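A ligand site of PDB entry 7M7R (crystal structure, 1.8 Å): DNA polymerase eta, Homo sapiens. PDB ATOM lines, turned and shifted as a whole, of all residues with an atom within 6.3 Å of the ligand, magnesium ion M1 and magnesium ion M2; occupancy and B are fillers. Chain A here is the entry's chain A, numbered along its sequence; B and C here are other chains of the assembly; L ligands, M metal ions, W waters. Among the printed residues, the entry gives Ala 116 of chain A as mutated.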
ATOM      1  N   ASP A  16     -13.917 -12.731 -15.066  1.00  0.00           N
ATOM      2  CA  ASP A  16     -14.954 -12.117 -14.236  1.00  0.00           C
ATOM      3  C   ASP A  16     -16.196 -11.831 -15.063  1.00  0.00           C
ATOM      4  O   ASP A  16     -16.125 -11.098 -16.063  1.00  0.00           O
ATOM      5  CB  ASP A  16     -14.437 -10.831 -13.591  1.00  0.00           C
ATOM      6  CG  ASP A  16     -15.428 -10.257 -12.618  1.00  0.00           C
ATOM      7  OD1 ASP A  16     -16.455  -9.743 -13.074  1.00  0.00           O
ATOM      8  OD2 ASP A  16     -15.207 -10.355 -11.398  1.00  0.00           O
ATOM      9  N   MET A  17     -17.344 -12.357 -14.632  1.00  0.00           N
ATOM     10  CA  MET A  17     -18.578 -12.172 -15.388  1.00  0.00           C
ATOM     11  C   MET A  17     -18.984 -10.697 -15.385  1.00  0.00           C
ATOM     12  O   MET A  17     -18.802  -9.989 -14.391  1.00  0.00           O
ATOM     13  CB  MET A  17     -19.692 -13.015 -14.774  1.00  0.00           C
ATOM     14  CG  MET A  17     -19.348 -14.494 -14.584  1.00  0.00           C
ATOM     15  SD  MET A  17     -18.731 -15.270 -16.087  1.00  0.00           S
ATOM     16  CE  MET A  17     -20.161 -15.163 -17.142  1.00  0.00           C
ATOM     17  N   ASP A  18     -19.516 -10.229 -16.509  1.00  0.00           N
ATOM     18  CA  ASP A  18     -20.023  -8.861 -16.585  1.00  0.00           C
ATOM     19  C   ASP A  18     -21.394  -8.778 -15.913  1.00  0.00           C
ATOM     20  O   ASP A  18     -22.266  -9.610 -16.189  1.00  0.00           O
ATOM     21  CB  ASP A  18     -20.118  -8.419 -18.039  1.00  0.00           C
ATOM     22  CG  ASP A  18     -18.755  -8.428 -18.758  1.00  0.00           C
ATOM     23  OD1 ASP A  18     -17.703  -8.213 -18.102  1.00  0.00           O
ATOM     24  OD2 ASP A  18     -18.742  -8.612 -19.989  1.00  0.00           O
ATOM     25  N   CYS A  19     -21.582  -7.741 -15.083  1.00  0.00           N
ATOM     26  CA  CYS A  19     -22.820  -7.471 -14.321  1.00  0.00           C
ATOM     27  C   CYS A  19     -23.571  -8.766 -14.069  1.00  0.00           C
ATOM     28  O   CYS A  19     -24.699  -8.962 -14.558  1.00  0.00           O
ATOM     29  CB  CYS A  19     -23.709  -6.438 -15.029  1.00  0.00           C
ATOM     30  SG  CYS A  19     -24.112  -6.759 -16.771  1.00  0.00           S
ATOM     31  N   PHE A  20     -22.927  -9.670 -13.314  1.00  0.00           N
ATOM     32  CA  PHE A  20     -23.324 -11.076 -13.281  1.00  0.00           C
ATOM     33  C   PHE A  20     -24.787 -11.319 -12.920  1.00  0.00           C
ATOM     34  O   PHE A  20     -25.510 -12.022 -13.648  1.00  0.00           O
ATOM     35  CB  PHE A  20     -22.392 -11.863 -12.372  1.00  0.00           C
ATOM     36  CG  PHE A  20     -22.662 -13.325 -12.414  1.00  0.00           C
ATOM     37  CD1 PHE A  20     -22.783 -13.990 -13.627  1.00  0.00           C
ATOM     38  CD2 PHE A  20     -22.769 -14.049 -11.237  1.00  0.00           C
ATOM     39  CE1 PHE A  20     -23.031 -15.354 -13.668  1.00  0.00           C
ATOM     40  CE2 PHE A  20     -23.012 -15.432 -11.275  1.00  0.00           C
ATOM     41  CZ  PHE A  20     -23.137 -16.078 -12.491  1.00  0.00           C
ATOM     42  N   PHE A  21     -25.241 -10.809 -11.768  1.00  0.00           N
ATOM     43  CA  PHE A  21     -26.604 -11.147 -11.356  1.00  0.00           C
ATOM     44  C   PHE A  21     -27.601 -10.598 -12.373  1.00  0.00           C
ATOM     45  O   PHE A  21     -28.658 -11.206 -12.608  1.00  0.00           O
ATOM     46  CB  PHE A  21     -26.924 -10.611  -9.955  1.00  0.00           C
ATOM     47  CG  PHE A  21     -26.228 -11.333  -8.825  1.00  0.00           C
ATOM     48  CD1 PHE A  21     -25.168 -12.194  -9.068  1.00  0.00           C
ATOM     49  CD2 PHE A  21     -26.627 -11.137  -7.511  1.00  0.00           C
ATOM     50  CE1 PHE A  21     -24.506 -12.833  -8.023  1.00  0.00           C
ATOM     51  CE2 PHE A  21     -25.972 -11.774  -6.445  1.00  0.00           C
ATOM     52  CZ  PHE A  21     -24.916 -12.618  -6.705  1.00  0.00           C
ATOM     53  N   VAL A  22     -27.276  -9.450 -12.978  1.00  0.00           N
ATOM     54  CA  VAL A  22     -28.140  -8.883 -14.003  1.00  0.00           C
ATOM     55  C   VAL A  22     -28.224  -9.819 -15.211  1.00  0.00           C
ATOM     56  O   VAL A  22     -29.315 -10.084 -15.725  1.00  0.00           O
ATOM     57  CB  VAL A  22     -27.621  -7.487 -14.411  1.00  0.00           C
ATOM     58  CG1 VAL A  22     -28.277  -7.021 -15.716  1.00  0.00           C
ATOM     59  CG2 VAL A  22     -27.804  -6.494 -13.267  1.00  0.00           C
ATOM     60  N   GLN A  41     -32.308  -6.282  -3.626  1.00  0.00           N
ATOM     61  CA  GLN A  41     -32.734  -7.138  -2.523  1.00  0.00           C
ATOM     62  C   GLN A  41     -33.714  -6.380  -1.641  1.00  0.00           C
ATOM     63  O   GLN A  41     -33.448  -5.223  -1.283  1.00  0.00           O
ATOM     64  CB  GLN A  41     -31.531  -7.508  -1.641  1.00  0.00           C
ATOM     65  CG  GLN A  41     -30.442  -8.292  -2.303  1.00  0.00           C
ATOM     66  CD  GLN A  41     -29.427  -8.786  -1.292  1.00  0.00           C
ATOM     67  OE1 GLN A  41     -29.153  -9.982  -1.182  1.00  0.00           O
ATOM     68  NE2 GLN A  41     -28.834  -7.851  -0.552  1.00  0.00           N
ATOM     69  N   ILE A  51     -27.779  -4.508  -5.874  1.00  0.00           N
ATOM     70  CA  ILE A  51     -26.543  -5.264  -5.749  1.00  0.00           C
ATOM     71  C   ILE A  51     -25.872  -5.518  -7.091  1.00  0.00           C
ATOM     72  O   ILE A  51     -24.707  -5.951  -7.116  1.00  0.00           O
ATOM     73  CB  ILE A  51     -26.732  -6.596  -4.979  1.00  0.00           C
ATOM     74  CG1 ILE A  51     -27.742  -7.510  -5.667  1.00  0.00           C
ATOM     75  CG2 ILE A  51     -27.123  -6.295  -3.523  1.00  0.00           C
ATOM     76  CD1 ILE A  51     -27.816  -8.875  -5.011  1.00  0.00           C
ATOM     77  N   ALA A  52     -26.550  -5.277  -8.207  1.00  0.00           N
ATOM     78  CA  ALA A  52     -25.891  -5.435  -9.513  1.00  0.00           C
ATOM     79  C   ALA A  52     -26.575  -4.528 -10.533  1.00  0.00           C
ATOM     80  O   ALA A  52     -27.776  -4.290 -10.445  1.00  0.00           O
ATOM     81  CB  ALA A  52     -25.954  -6.904  -9.970  1.00  0.00           C
ATOM     82  N   VAL A  53     -25.795  -4.030 -11.504  1.00  0.00           N
ATOM     83  CA  VAL A  53     -26.259  -2.962 -12.394  1.00  0.00           C
ATOM     84  C   VAL A  53     -25.754  -3.221 -13.803  1.00  0.00           C
ATOM     85  O   VAL A  53     -24.542  -3.412 -14.005  1.00  0.00           O
ATOM     86  CB  VAL A  53     -25.751  -1.577 -11.907  1.00  0.00           C
ATOM     87  CG1 VAL A  53     -26.349  -0.460 -12.756  1.00  0.00           C
ATOM     88  CG2 VAL A  53     -26.063  -1.341 -10.447  1.00  0.00           C
ATOM     89  N   TYR A  55     -24.670  -2.385 -17.690  1.00  0.00           N
ATOM     90  CA  TYR A  55     -23.844  -1.275 -18.178  1.00  0.00           C
ATOM     91  C   TYR A  55     -24.696  -0.140 -18.743  1.00  0.00           C
ATOM     92  O   TYR A  55     -24.365   1.045 -18.574  1.00  0.00           O
ATOM     93  CB  TYR A  55     -22.829  -1.798 -19.194  1.00  0.00           C
ATOM     94  CG  TYR A  55     -21.672  -2.466 -18.506  1.00  0.00           C
ATOM     95  CD1 TYR A  55     -21.792  -3.759 -17.989  1.00  0.00           C
ATOM     96  CD2 TYR A  55     -20.504  -1.767 -18.239  1.00  0.00           C
ATOM     97  CE1 TYR A  55     -20.761  -4.349 -17.294  1.00  0.00           C
ATOM     98  CE2 TYR A  55     -19.449  -2.364 -17.549  1.00  0.00           C
ATOM     99  CZ  TYR A  55     -19.587  -3.646 -17.078  1.00  0.00           C
ATOM    100  OH  TYR A  55     -18.539  -4.243 -16.380  1.00  0.00           O
ATOM    101  N   ARG A  58     -25.504   1.787 -15.727  1.00  0.00           N
ATOM    102  CA  ARG A  58     -24.355   2.485 -15.168  1.00  0.00           C
ATOM    103  C   ARG A  58     -24.112   3.803 -15.900  1.00  0.00           C
ATOM    104  O   ARG A  58     -23.620   4.766 -15.301  1.00  0.00           O
ATOM    105  CB  ARG A  58     -23.096   1.616 -15.270  1.00  0.00           C
ATOM    106  CG  ARG A  58     -23.191   0.351 -14.471  1.00  0.00           C
ATOM    107  CD  ARG A  58     -21.954  -0.522 -14.637  1.00  0.00           C
ATOM    108  NE  ARG A  58     -22.209  -1.899 -14.204  1.00  0.00           N
ATOM    109  CZ  ARG A  58     -21.264  -2.778 -13.925  1.00  0.00           C
ATOM    110  NH1 ARG A  58     -19.977  -2.441 -14.032  1.00  0.00           N
ATOM    111  NH2 ARG A  58     -21.600  -4.013 -13.537  1.00  0.00           N
ATOM    112  N   ARG A  64     -24.034  -0.059  -7.509  1.00  0.00           N
ATOM    113  CA  ARG A  64     -24.247  -0.925  -6.365  1.00  0.00           C
ATOM    114  C   ARG A  64     -24.376  -0.107  -5.079  1.00  0.00           C
ATOM    115  O   ARG A  64     -23.725   0.938  -4.926  1.00  0.00           O
ATOM    116  CB  ARG A  64     -23.077  -1.913  -6.236  1.00  0.00           C
ATOM    117  CG  ARG A  64     -22.986  -2.607  -4.874  1.00  0.00           C
ATOM    118  CD  ARG A  64     -21.758  -3.494  -4.709  1.00  0.00           C
ATOM    119  NE  ARG A  64     -20.515  -2.743  -4.478  1.00  0.00           N
ATOM    120  CZ  ARG A  64     -20.143  -2.236  -3.307  1.00  0.00           C
ATOM    121  NH1 ARG A  64     -18.997  -1.577  -3.207  1.00  0.00           N
ATOM    122  NH2 ARG A  64     -20.926  -2.348  -2.243  1.00  0.00           N
ATOM    123  N   ALA A 116     -14.551 -15.831  -6.361  1.00  0.00           N
ATOM    124  CA  ALA A 116     -15.817 -15.306  -5.851  1.00  0.00           C
ATOM    125  C   ALA A 116     -16.932 -15.875  -6.707  1.00  0.00           C
ATOM    126  O   ALA A 116     -16.676 -16.600  -7.689  1.00  0.00           O
ATOM    127  CB  ALA A 116     -15.844 -13.780  -5.847  1.00  0.00           C
ATOM    128  N   ILE A 117     -18.174 -15.507  -6.381  1.00  0.00           N
ATOM    129  CA  ILE A 117     -19.319 -16.097  -7.056  1.00  0.00           C
ATOM    130  C   ILE A 117     -19.231 -15.935  -8.572  1.00  0.00           C
ATOM    131  O   ILE A 117     -19.726 -16.787  -9.309  1.00  0.00           O
ATOM    132  CB  ILE A 117     -20.649 -15.509  -6.522  1.00  0.00           C
ATOM    133  CG1 ILE A 117     -21.836 -16.396  -6.975  1.00  0.00           C
ATOM    134  CG2 ILE A 117     -20.817 -14.084  -6.978  1.00  0.00           C
ATOM    135  CD1 ILE A 117     -23.085 -16.238  -6.118  1.00  0.00           C
ATOM    136  N   ASP A 118     -18.523 -14.915  -9.071  1.00  0.00           N
ATOM    137  CA  ASP A 118     -18.531 -14.711 -10.510  1.00  0.00           C
ATOM    138  C   ASP A 118     -17.129 -14.596 -11.082  1.00  0.00           C
ATOM    139  O   ASP A 118     -16.969 -14.111 -12.207  1.00  0.00           O
ATOM    140  CB  ASP A 118     -19.330 -13.440 -10.871  1.00  0.00           C
ATOM    141  CG  ASP A 118     -18.477 -12.167 -10.868  1.00  0.00           C
ATOM    142  OD1 ASP A 118     -17.615 -11.997  -9.966  1.00  0.00           O
ATOM    143  OD2 ASP A 118     -18.683 -11.326 -11.783  1.00  0.00           O
ATOM    144  N   GLU A 119     -16.107 -15.068 -10.346  1.00  0.00           N
ATOM    145  CA  GLU A 119     -14.766 -15.009 -10.926  1.00  0.00           C
ATOM    146  C   GLU A 119     -13.865 -16.144 -10.496  1.00  0.00           C
ATOM    147  O   GLU A 119     -13.953 -16.653  -9.358  1.00  0.00           O
ATOM    148  CB  GLU A 119     -14.057 -13.691 -10.625  1.00  0.00           C
ATOM    149  CG  GLU A 119     -13.639 -13.521  -9.218  1.00  0.00           C
ATOM    150  CD  GLU A 119     -13.504 -12.059  -8.915  1.00  0.00           C
ATOM    151  OE1 GLU A 119     -12.367 -11.564  -8.991  1.00  0.00           O
ATOM    152  OE2 GLU A 119     -14.537 -11.389  -8.743  1.00  0.00           O
ATOM    153  N   LYS A 227      -6.000  -9.883 -12.450  1.00  0.00           N
ATOM    154  CA  LYS A 227      -7.187  -9.222 -11.908  1.00  0.00           C
ATOM    155  C   LYS A 227      -7.234  -7.754 -12.325  1.00  0.00           C
ATOM    156  O   LYS A 227      -8.293  -7.224 -12.698  1.00  0.00           O
ATOM    157  CB  LYS A 227      -7.180  -9.351 -10.381  1.00  0.00           C
ATOM    158  CG  LYS A 227      -8.281  -8.577  -9.632  1.00  0.00           C
ATOM    159  CD  LYS A 227      -9.679  -9.060 -10.057  1.00  0.00           C
ATOM    160  CE  LYS A 227     -10.804  -8.534  -9.137  1.00  0.00           C
ATOM    161  NZ  LYS A 227     -12.151  -8.856  -9.727  1.00  0.00           N
ATOM    162  N   LYS A 234     -13.436  -3.991 -19.457  1.00  0.00           N
ATOM    163  CA  LYS A 234     -14.828  -4.400 -19.263  1.00  0.00           C
ATOM    164  C   LYS A 234     -15.788  -3.404 -19.917  1.00  0.00           C
ATOM    165  O   LYS A 234     -15.566  -2.190 -19.869  1.00  0.00           O
ATOM    166  CB  LYS A 234     -15.155  -4.461 -17.767  1.00  0.00           C
ATOM    167  CG  LYS A 234     -14.917  -5.801 -17.122  1.00  0.00           C
ATOM    168  CD  LYS A 234     -15.450  -5.845 -15.691  1.00  0.00           C
ATOM    169  CE  LYS A 234     -15.376  -7.265 -15.130  1.00  0.00           C
ATOM    170  NZ  LYS A 234     -16.589  -8.066 -15.532  1.00  0.00           N
ATOM    171  N   PRO A 235     -16.911  -3.890 -20.478  1.00  0.00           N
ATOM    172  CA  PRO A 235     -17.260  -5.320 -20.469  1.00  0.00           C
ATOM    173  C   PRO A 235     -16.953  -6.061 -21.769  1.00  0.00           C
ATOM    174  O   PRO A 235     -16.620  -5.438 -22.782  1.00  0.00           O
ATOM    175  CB  PRO A 235     -18.768  -5.296 -20.263  1.00  0.00           C
ATOM    176  CG  PRO A 235     -19.186  -4.071 -21.067  1.00  0.00           C
ATOM    177  CD  PRO A 235     -18.063  -3.066 -20.897  1.00  0.00           C
ATOM    178  P     A B   8     -13.384  -6.927  -5.749  1.00  0.00           P
ATOM    179  OP1   A B   8     -12.740  -7.053  -7.096  1.00  0.00           O
ATOM    180  OP2   A B   8     -14.003  -5.650  -5.307  1.00  0.00           O
ATOM    181  O5'   A B   8     -14.503  -8.063  -5.557  1.00  0.00           O
ATOM    182  C5'   A B   8     -14.339  -9.438  -5.923  1.00  0.00           C
ATOM    183  C4'   A B   8     -15.644 -10.184  -5.692  1.00  0.00           C
ATOM    184  O4'   A B   8     -15.995 -10.140  -4.284  1.00  0.00           O
ATOM    185  C3'   A B   8     -16.855  -9.605  -6.412  1.00  0.00           C
ATOM    186  O3'   A B   8     -17.005 -10.205  -7.692  1.00  0.00           O
ATOM    187  C2'   A B   8     -18.043  -9.923  -5.498  1.00  0.00           C
ATOM    188  O2'   A B   8     -18.584 -11.183  -5.868  1.00  0.00           O
ATOM    189  C1'   A B   8     -17.386 -10.055  -4.113  1.00  0.00           C
ATOM    190  N9    A B   8     -17.680  -8.988  -3.132  1.00  0.00           N
ATOM    191  C8    A B   8     -17.005  -7.818  -2.875  1.00  0.00           C
ATOM    192  N7    A B   8     -17.478  -7.125  -1.857  1.00  0.00           N
ATOM    193  C5    A B   8     -18.521  -7.901  -1.381  1.00  0.00           C
ATOM    194  C6    A B   8     -19.435  -7.742  -0.316  1.00  0.00           C
ATOM    195  N6    A B   8     -19.464  -6.701   0.517  1.00  0.00           N
ATOM    196  N1    A B   8     -20.346  -8.707  -0.116  1.00  0.00           N
ATOM    197  C2    A B   8     -20.347  -9.774  -0.938  1.00  0.00           C
ATOM    198  N3    A B   8     -19.546 -10.045  -1.967  1.00  0.00           N
ATOM    199  C4    A B   8     -18.640  -9.057  -2.143  1.00  0.00           C
ATOM    200  P    DT C   3     -27.446   3.097   5.162  1.00  0.00           P
ATOM    201  OP1  DT C   3     -26.771   3.642   6.355  1.00  0.00           O
ATOM    202  OP2  DT C   3     -27.559   3.901   3.940  1.00  0.00           O
ATOM    203  O5'  DT C   3     -26.738   1.748   4.733  1.00  0.00           O
ATOM    204  C5'  DT C   3     -26.905   1.292   3.402  1.00  0.00           C
ATOM    205  C4'  DT C   3     -27.574  -0.064   3.407  1.00  0.00           C
ATOM    206  O4'  DT C   3     -27.097  -0.814   2.277  1.00  0.00           O
ATOM    207  C3'  DT C   3     -27.298  -0.948   4.616  1.00  0.00           C
ATOM    208  O3'  DT C   3     -28.510  -1.655   4.900  1.00  0.00           O
ATOM    209  C2'  DT C   3     -26.108  -1.787   4.194  1.00  0.00           C
ATOM    210  C1'  DT C   3     -26.053  -1.673   2.684  1.00  0.00           C
ATOM    211  N1   DT C   3     -24.795  -1.124   2.181  1.00  0.00           N
ATOM    212  C2   DT C   3     -24.401  -1.527   0.934  1.00  0.00           C
ATOM    213  O2   DT C   3     -25.049  -2.310   0.248  1.00  0.00           O
ATOM    214  N3   DT C   3     -23.203  -0.999   0.511  1.00  0.00           N
ATOM    215  C4   DT C   3     -22.396  -0.119   1.193  1.00  0.00           C
ATOM    216  O4   DT C   3     -21.358   0.276   0.672  1.00  0.00           O
ATOM    217  C5   DT C   3     -22.866   0.275   2.490  1.00  0.00           C
ATOM    218  C7   DT C   3     -22.050   1.219   3.313  1.00  0.00           C
ATOM    219  C6   DT C   3     -24.022  -0.252   2.928  1.00  0.00           C
ATOM    220  P    DT C   4     -28.536  -3.004   5.734  1.00  0.00           P
ATOM    221  OP1  DT C   4     -29.905  -3.208   6.220  1.00  0.00           O
ATOM    222  OP2  DT C   4     -27.409  -3.016   6.690  1.00  0.00           O
ATOM    223  O5'  DT C   4     -28.299  -4.114   4.623  1.00  0.00           O
ATOM    224  C5'  DT C   4     -29.288  -4.369   3.616  1.00  0.00           C
ATOM    225  C4'  DT C   4     -29.044  -5.722   3.006  1.00  0.00           C
ATOM    226  O4'  DT C   4     -27.924  -5.656   2.106  1.00  0.00           O
ATOM    227  C3'  DT C   4     -28.691  -6.805   4.023  1.00  0.00           C
ATOM    228  O3'  DT C   4     -29.399  -7.995   3.675  1.00  0.00           O
ATOM    229  C2'  DT C   4     -27.200  -7.014   3.844  1.00  0.00           C
ATOM    230  C1'  DT C   4     -27.027  -6.712   2.381  1.00  0.00           C
ATOM    231  N1   DT C   4     -25.686  -6.271   1.995  1.00  0.00           N
ATOM    232  C2   DT C   4     -25.192  -6.767   0.814  1.00  0.00           C
ATOM    233  O2   DT C   4     -25.794  -7.563   0.117  1.00  0.00           O
ATOM    234  N3   DT C   4     -23.942  -6.305   0.495  1.00  0.00           N
ATOM    235  C4   DT C   4     -23.167  -5.408   1.202  1.00  0.00           C
ATOM    236  O4   DT C   4     -22.062  -5.085   0.786  1.00  0.00           O
ATOM    237  C5   DT C   4     -23.766  -4.927   2.434  1.00  0.00           C
ATOM    238  C7   DT C   4     -22.996  -3.968   3.282  1.00  0.00           C
ATOM    239  C6   DT C   4     -24.984  -5.371   2.758  1.00  0.00           C
ATOM    240  P    DT C   5     -29.320  -9.357   4.542  1.00  0.00           P
ATOM    241  OP1  DT C   5     -30.658  -9.962   4.522  1.00  0.00           O
ATOM    242  OP2  DT C   5     -28.638  -9.076   5.824  1.00  0.00           O
ATOM    243  O5'  DT C   5     -28.325 -10.281   3.706  1.00  0.00           O
ATOM    244  C5'  DT C   5     -28.623 -10.632   2.364  1.00  0.00           C
ATOM    245  C4'  DT C   5     -27.502 -11.458   1.788  1.00  0.00           C
ATOM    246  O4'  DT C   5     -26.331 -10.630   1.542  1.00  0.00           O
ATOM    247  C3'  DT C   5     -27.031 -12.594   2.695  1.00  0.00           C
ATOM    248  O3'  DT C   5     -26.798 -13.737   1.917  1.00  0.00           O
ATOM    249  C2'  DT C   5     -25.719 -12.043   3.279  1.00  0.00           C
ATOM    250  C1'  DT C   5     -25.197 -11.265   2.068  1.00  0.00           C
ATOM    251  N1   DT C   5     -24.181 -10.229   2.389  1.00  0.00           N
ATOM    252  C2   DT C   5     -23.144 -10.013   1.501  1.00  0.00           C
ATOM    253  O2   DT C   5     -23.002 -10.646   0.468  1.00  0.00           O
ATOM    254  N3   DT C   5     -22.268  -9.033   1.862  1.00  0.00           N
ATOM    255  C4   DT C   5     -22.324  -8.253   2.990  1.00  0.00           C
ATOM    256  O4   DT C   5     -21.474  -7.392   3.219  1.00  0.00           O
ATOM    257  C5   DT C   5     -23.431  -8.513   3.891  1.00  0.00           C
ATOM    258  C7   DT C   5     -23.585  -7.714   5.149  1.00  0.00           C
ATOM    259  C6   DT C   5     -24.294  -9.489   3.543  1.00  0.00           C
HETATM  260  N1  LIG L   1     -22.971  -7.186  -1.863  1.00  0.00           N
HETATM  261  C1  LIG L   1     -23.681  -8.177  -2.398  1.00  0.00           C
HETATM  262  N2  LIG L   1     -23.530  -8.760  -3.589  1.00  0.00           N
HETATM  263  C2  LIG L   1     -22.515  -8.196  -4.264  1.00  0.00           C
HETATM  264  C3  LIG L   1     -21.706  -7.171  -3.853  1.00  0.00           C
HETATM  265  C4  LIG L   1     -21.958  -6.648  -2.570  1.00  0.00           C
HETATM  266  N3  LIG L   1     -21.237  -5.648  -2.065  1.00  0.00           N
HETATM  267  N4  LIG L   1     -20.775  -6.867  -4.828  1.00  0.00           N
HETATM  268  C5  LIG L   1     -21.042  -7.715  -5.803  1.00  0.00           C
HETATM  269  N5  LIG L   1     -22.084  -8.540  -5.512  1.00  0.00           N
HETATM  270  P1  LIG L   1     -18.787  -8.064  -9.362  1.00  0.00           P
HETATM  271  P2  LIG L   1     -20.637  -7.436 -11.497  1.00  0.00           P
HETATM  272  P3  LIG L   1     -18.814  -6.212 -13.345  1.00  0.00           P
HETATM  273  C6  LIG L   1     -22.677  -9.580  -6.330  1.00  0.00           C
HETATM  274  O1  LIG L   1     -17.970  -8.903 -10.200  1.00  0.00           O
HETATM  275  O2  LIG L   1     -20.362  -8.759 -12.018  1.00  0.00           O
HETATM  276  O3  LIG L   1     -17.973  -7.333 -12.876  1.00  0.00           O
HETATM  277  C7  LIG L   1     -23.575  -9.056  -7.449  1.00  0.00           C
HETATM  278  O4  LIG L   1     -17.905  -7.247  -8.383  1.00  0.00           O
HETATM  279  O5  LIG L   1     -22.168  -7.239 -11.274  1.00  0.00           O
HETATM  280  O6  LIG L   1     -19.155  -6.308 -14.782  1.00  0.00           O
HETATM  281  C8  LIG L   1     -22.644  -9.067  -8.657  1.00  0.00           C
HETATM  282  O7  LIG L   1     -23.335  -9.238  -9.884  1.00  0.00           O
HETATM  283  N6  LIG L   1     -19.789  -7.081 -10.172  1.00  0.00           N
HETATM  284  O8  LIG L   1     -20.188  -6.349 -12.547  1.00  0.00           O
HETATM  285  O9  LIG L   1     -18.244  -4.884 -12.984  1.00  0.00           O
HETATM  286  C9  LIG L   1     -21.752 -10.267  -8.368  1.00  0.00           C
HETATM  287  O10 LIG L   1     -21.641 -10.345  -6.931  1.00  0.00           O
HETATM  288  C10 LIG L   1     -20.370 -10.159  -8.961  1.00  0.00           C
HETATM  289  O11 LIG L   1     -19.713  -8.995  -8.438  1.00  0.00           O
HETATM  290 MG    MG M   1     -18.348  -9.359 -12.393  1.00  0.00          MG
HETATM  291 MG    MG M   2     -16.334 -10.315  -9.649  1.00  0.00          MG
HETATM  292  O   HOH W   1     -15.546  -6.924 -11.552  1.00  0.00           O
HETATM  293  O   HOH W   2     -24.958 -11.170  -3.309  1.00  0.00           O
HETATM  294  O   HOH W   3     -15.208  -8.517  -9.309  1.00  0.00           O
HETATM  295  O   HOH W   4     -23.088  -4.754 -11.166  1.00  0.00           O
HETATM  296  O   HOH W   5     -17.350  -4.579  -8.713  1.00  0.00           O
HETATM  297  O   HOH W   6     -21.885  -5.576  -8.359  1.00  0.00           O
HETATM  298  O   HOH W   7     -18.837  -3.549 -10.699  1.00  0.00           O
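N6 of A 8 of chain B lies close to a nitrogen (N3) of the ligand (3.3 Å). OH of Tyr 55 is in hydrogen-bond range of O6 of the ligand (2.7 Å). O4 of DT 4 of chain C lies within hydrogen-bond range of N3 of the ligand (3.0 Å). O6 of the ligand sits at hydrogen-bond distance from N of Cys 19 (2.8 Å). An oxygen (O9) of the ligand is in salt-bridge range of the guanidinium group of Arg 58, at 3.2 Å. An oxygen (O5) of the ligand is in hydrogen-bond range of the backbone NH (N) of Phe 20, at 3.3 Å. NZ of Lys 234 is in salt-bridge range of O6 of the ligand (3.2 Å). O7 of the ligand is in hydrogen-bond range of N of Phe 21 (3.1 Å).
Water W3 bridges the side-chain amino group of Lys 227 and an oxygen (O4) of the ligand. Water W4 lies within hydrogen-bond range of O5 of the ligand (2.7 Å), N of Val 53 (2.8 Å) and NH2 of Arg 58 (2.9 Å). Water W6 lies within hydrogen-bond range of the backbone carbonyl oxygen (O) of Ile 51 and a nitrogen (N6) of the ligand.
NZ of Lys 234 touches magnesium ion M1, 3.8 Å away. Within 4 Å of magnesium ion M1: Asp 16, Met 17, Asp 118 and Lys 234. The nearest printed residue that does not touch magnesium ion M1 is Asp 18 (4.4 Å).
Magnesium ion M1 is bound by the side-chain carboxylate (OD1) of Asp 16 (2.0 Å), the side-chain carboxylate (OD2) of Asp 118 (2.1 Å), an oxygen (O3) of the ligand (2.1 Å), an oxygen (O2) of the ligand (2.1 Å), the backbone carbonyl oxygen (O) of Met 17 (2.1 Å) and an oxygen (O1) of the ligand (2.3 Å). Magnesium ion M1 has six donor atoms within binding distance.
Magnesium ion M2 is bound by O3' of A 8 of chain B (2.1 Å), the side-chain carboxylate of Asp 16 (2.1 Å), the side-chain carboxylate of Asp 118 (2.1 Å), water W3 (2.1 Å), an oxygen (O1) of the ligand (2.2 Å) and the side-chain carboxylate of Glu 119 (2.3 Å). Magnesium ion M2 has six donor atoms within binding distance.
The nearest printed residue that does not touch magnesium ion M2 is Lys 227 (4.4 Å).
O of Asp 16 lies within hydrogen-bond range of NZ of Lys 234, at 3.1 Å. The side-chain carboxylate (OD2) of Asp 16 sits close to the side-chain amino group (NZ) of Lys 227, 3.8 Å away. The side-chain amino group of Lys 234 sits close to the backbone carbonyl oxygen of Met 17 (3.1 Å). OE1 of Glu 119 lies within salt-bridge range of NZ of Lys 227 (2.8 Å). The side-chain hydroxyl (OH) of Tyr 55 is in hydrogen-bond range of the guanidinium group (NH1) of Arg 58 (3.3 Å). O2 of DT 4 of chain C sits at hydrogen-bond distance from NE2 of Gln 41 (3.1 Å). The backbone carbonyl oxygen (O) of Val 53 sits at hydrogen-bond distance from the guanidinium group (NE) of Arg 58. The side-chain amino group of Lys 234 lies within salt-bridge range of the side-chain carboxylate of Asp 18 (2.8 Å).
A nitrogen (N3) of the ligand sits close to the guanidinium group of Arg 64 (3.3 Å). Asp 18 touches the ligand. O of Ile 51 touches C7 of the ligand (3.3 Å). Ala 52 touches the ligand (CB to O7, 3.5 Å). CG2 of Ile 117 touches O10 of the ligand, at 3.8 Å. DT 5 of chain C touches the ligand (O2 to C1, 3.8 Å). Hydrophobic or aromatic side chains within 4 Å of the ligand: Phe 20, Phe 21, Ala 52, Tyr 55 and Ile 117. Within 4 Å of the ligand: Asp 16, Met 17, Asp 18, Cys 19, Phe 20, Phe 21, Ile 51, Ala 52, Tyr 55, Arg 58, Arg 64, Ile 117, Asp 118, Lys 234, A 8 of chain B, DT 4 of chain C and DT 5 of chain C. The nearest printed residue that does not touch the ligand is Glu 119 (4.5 Å).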
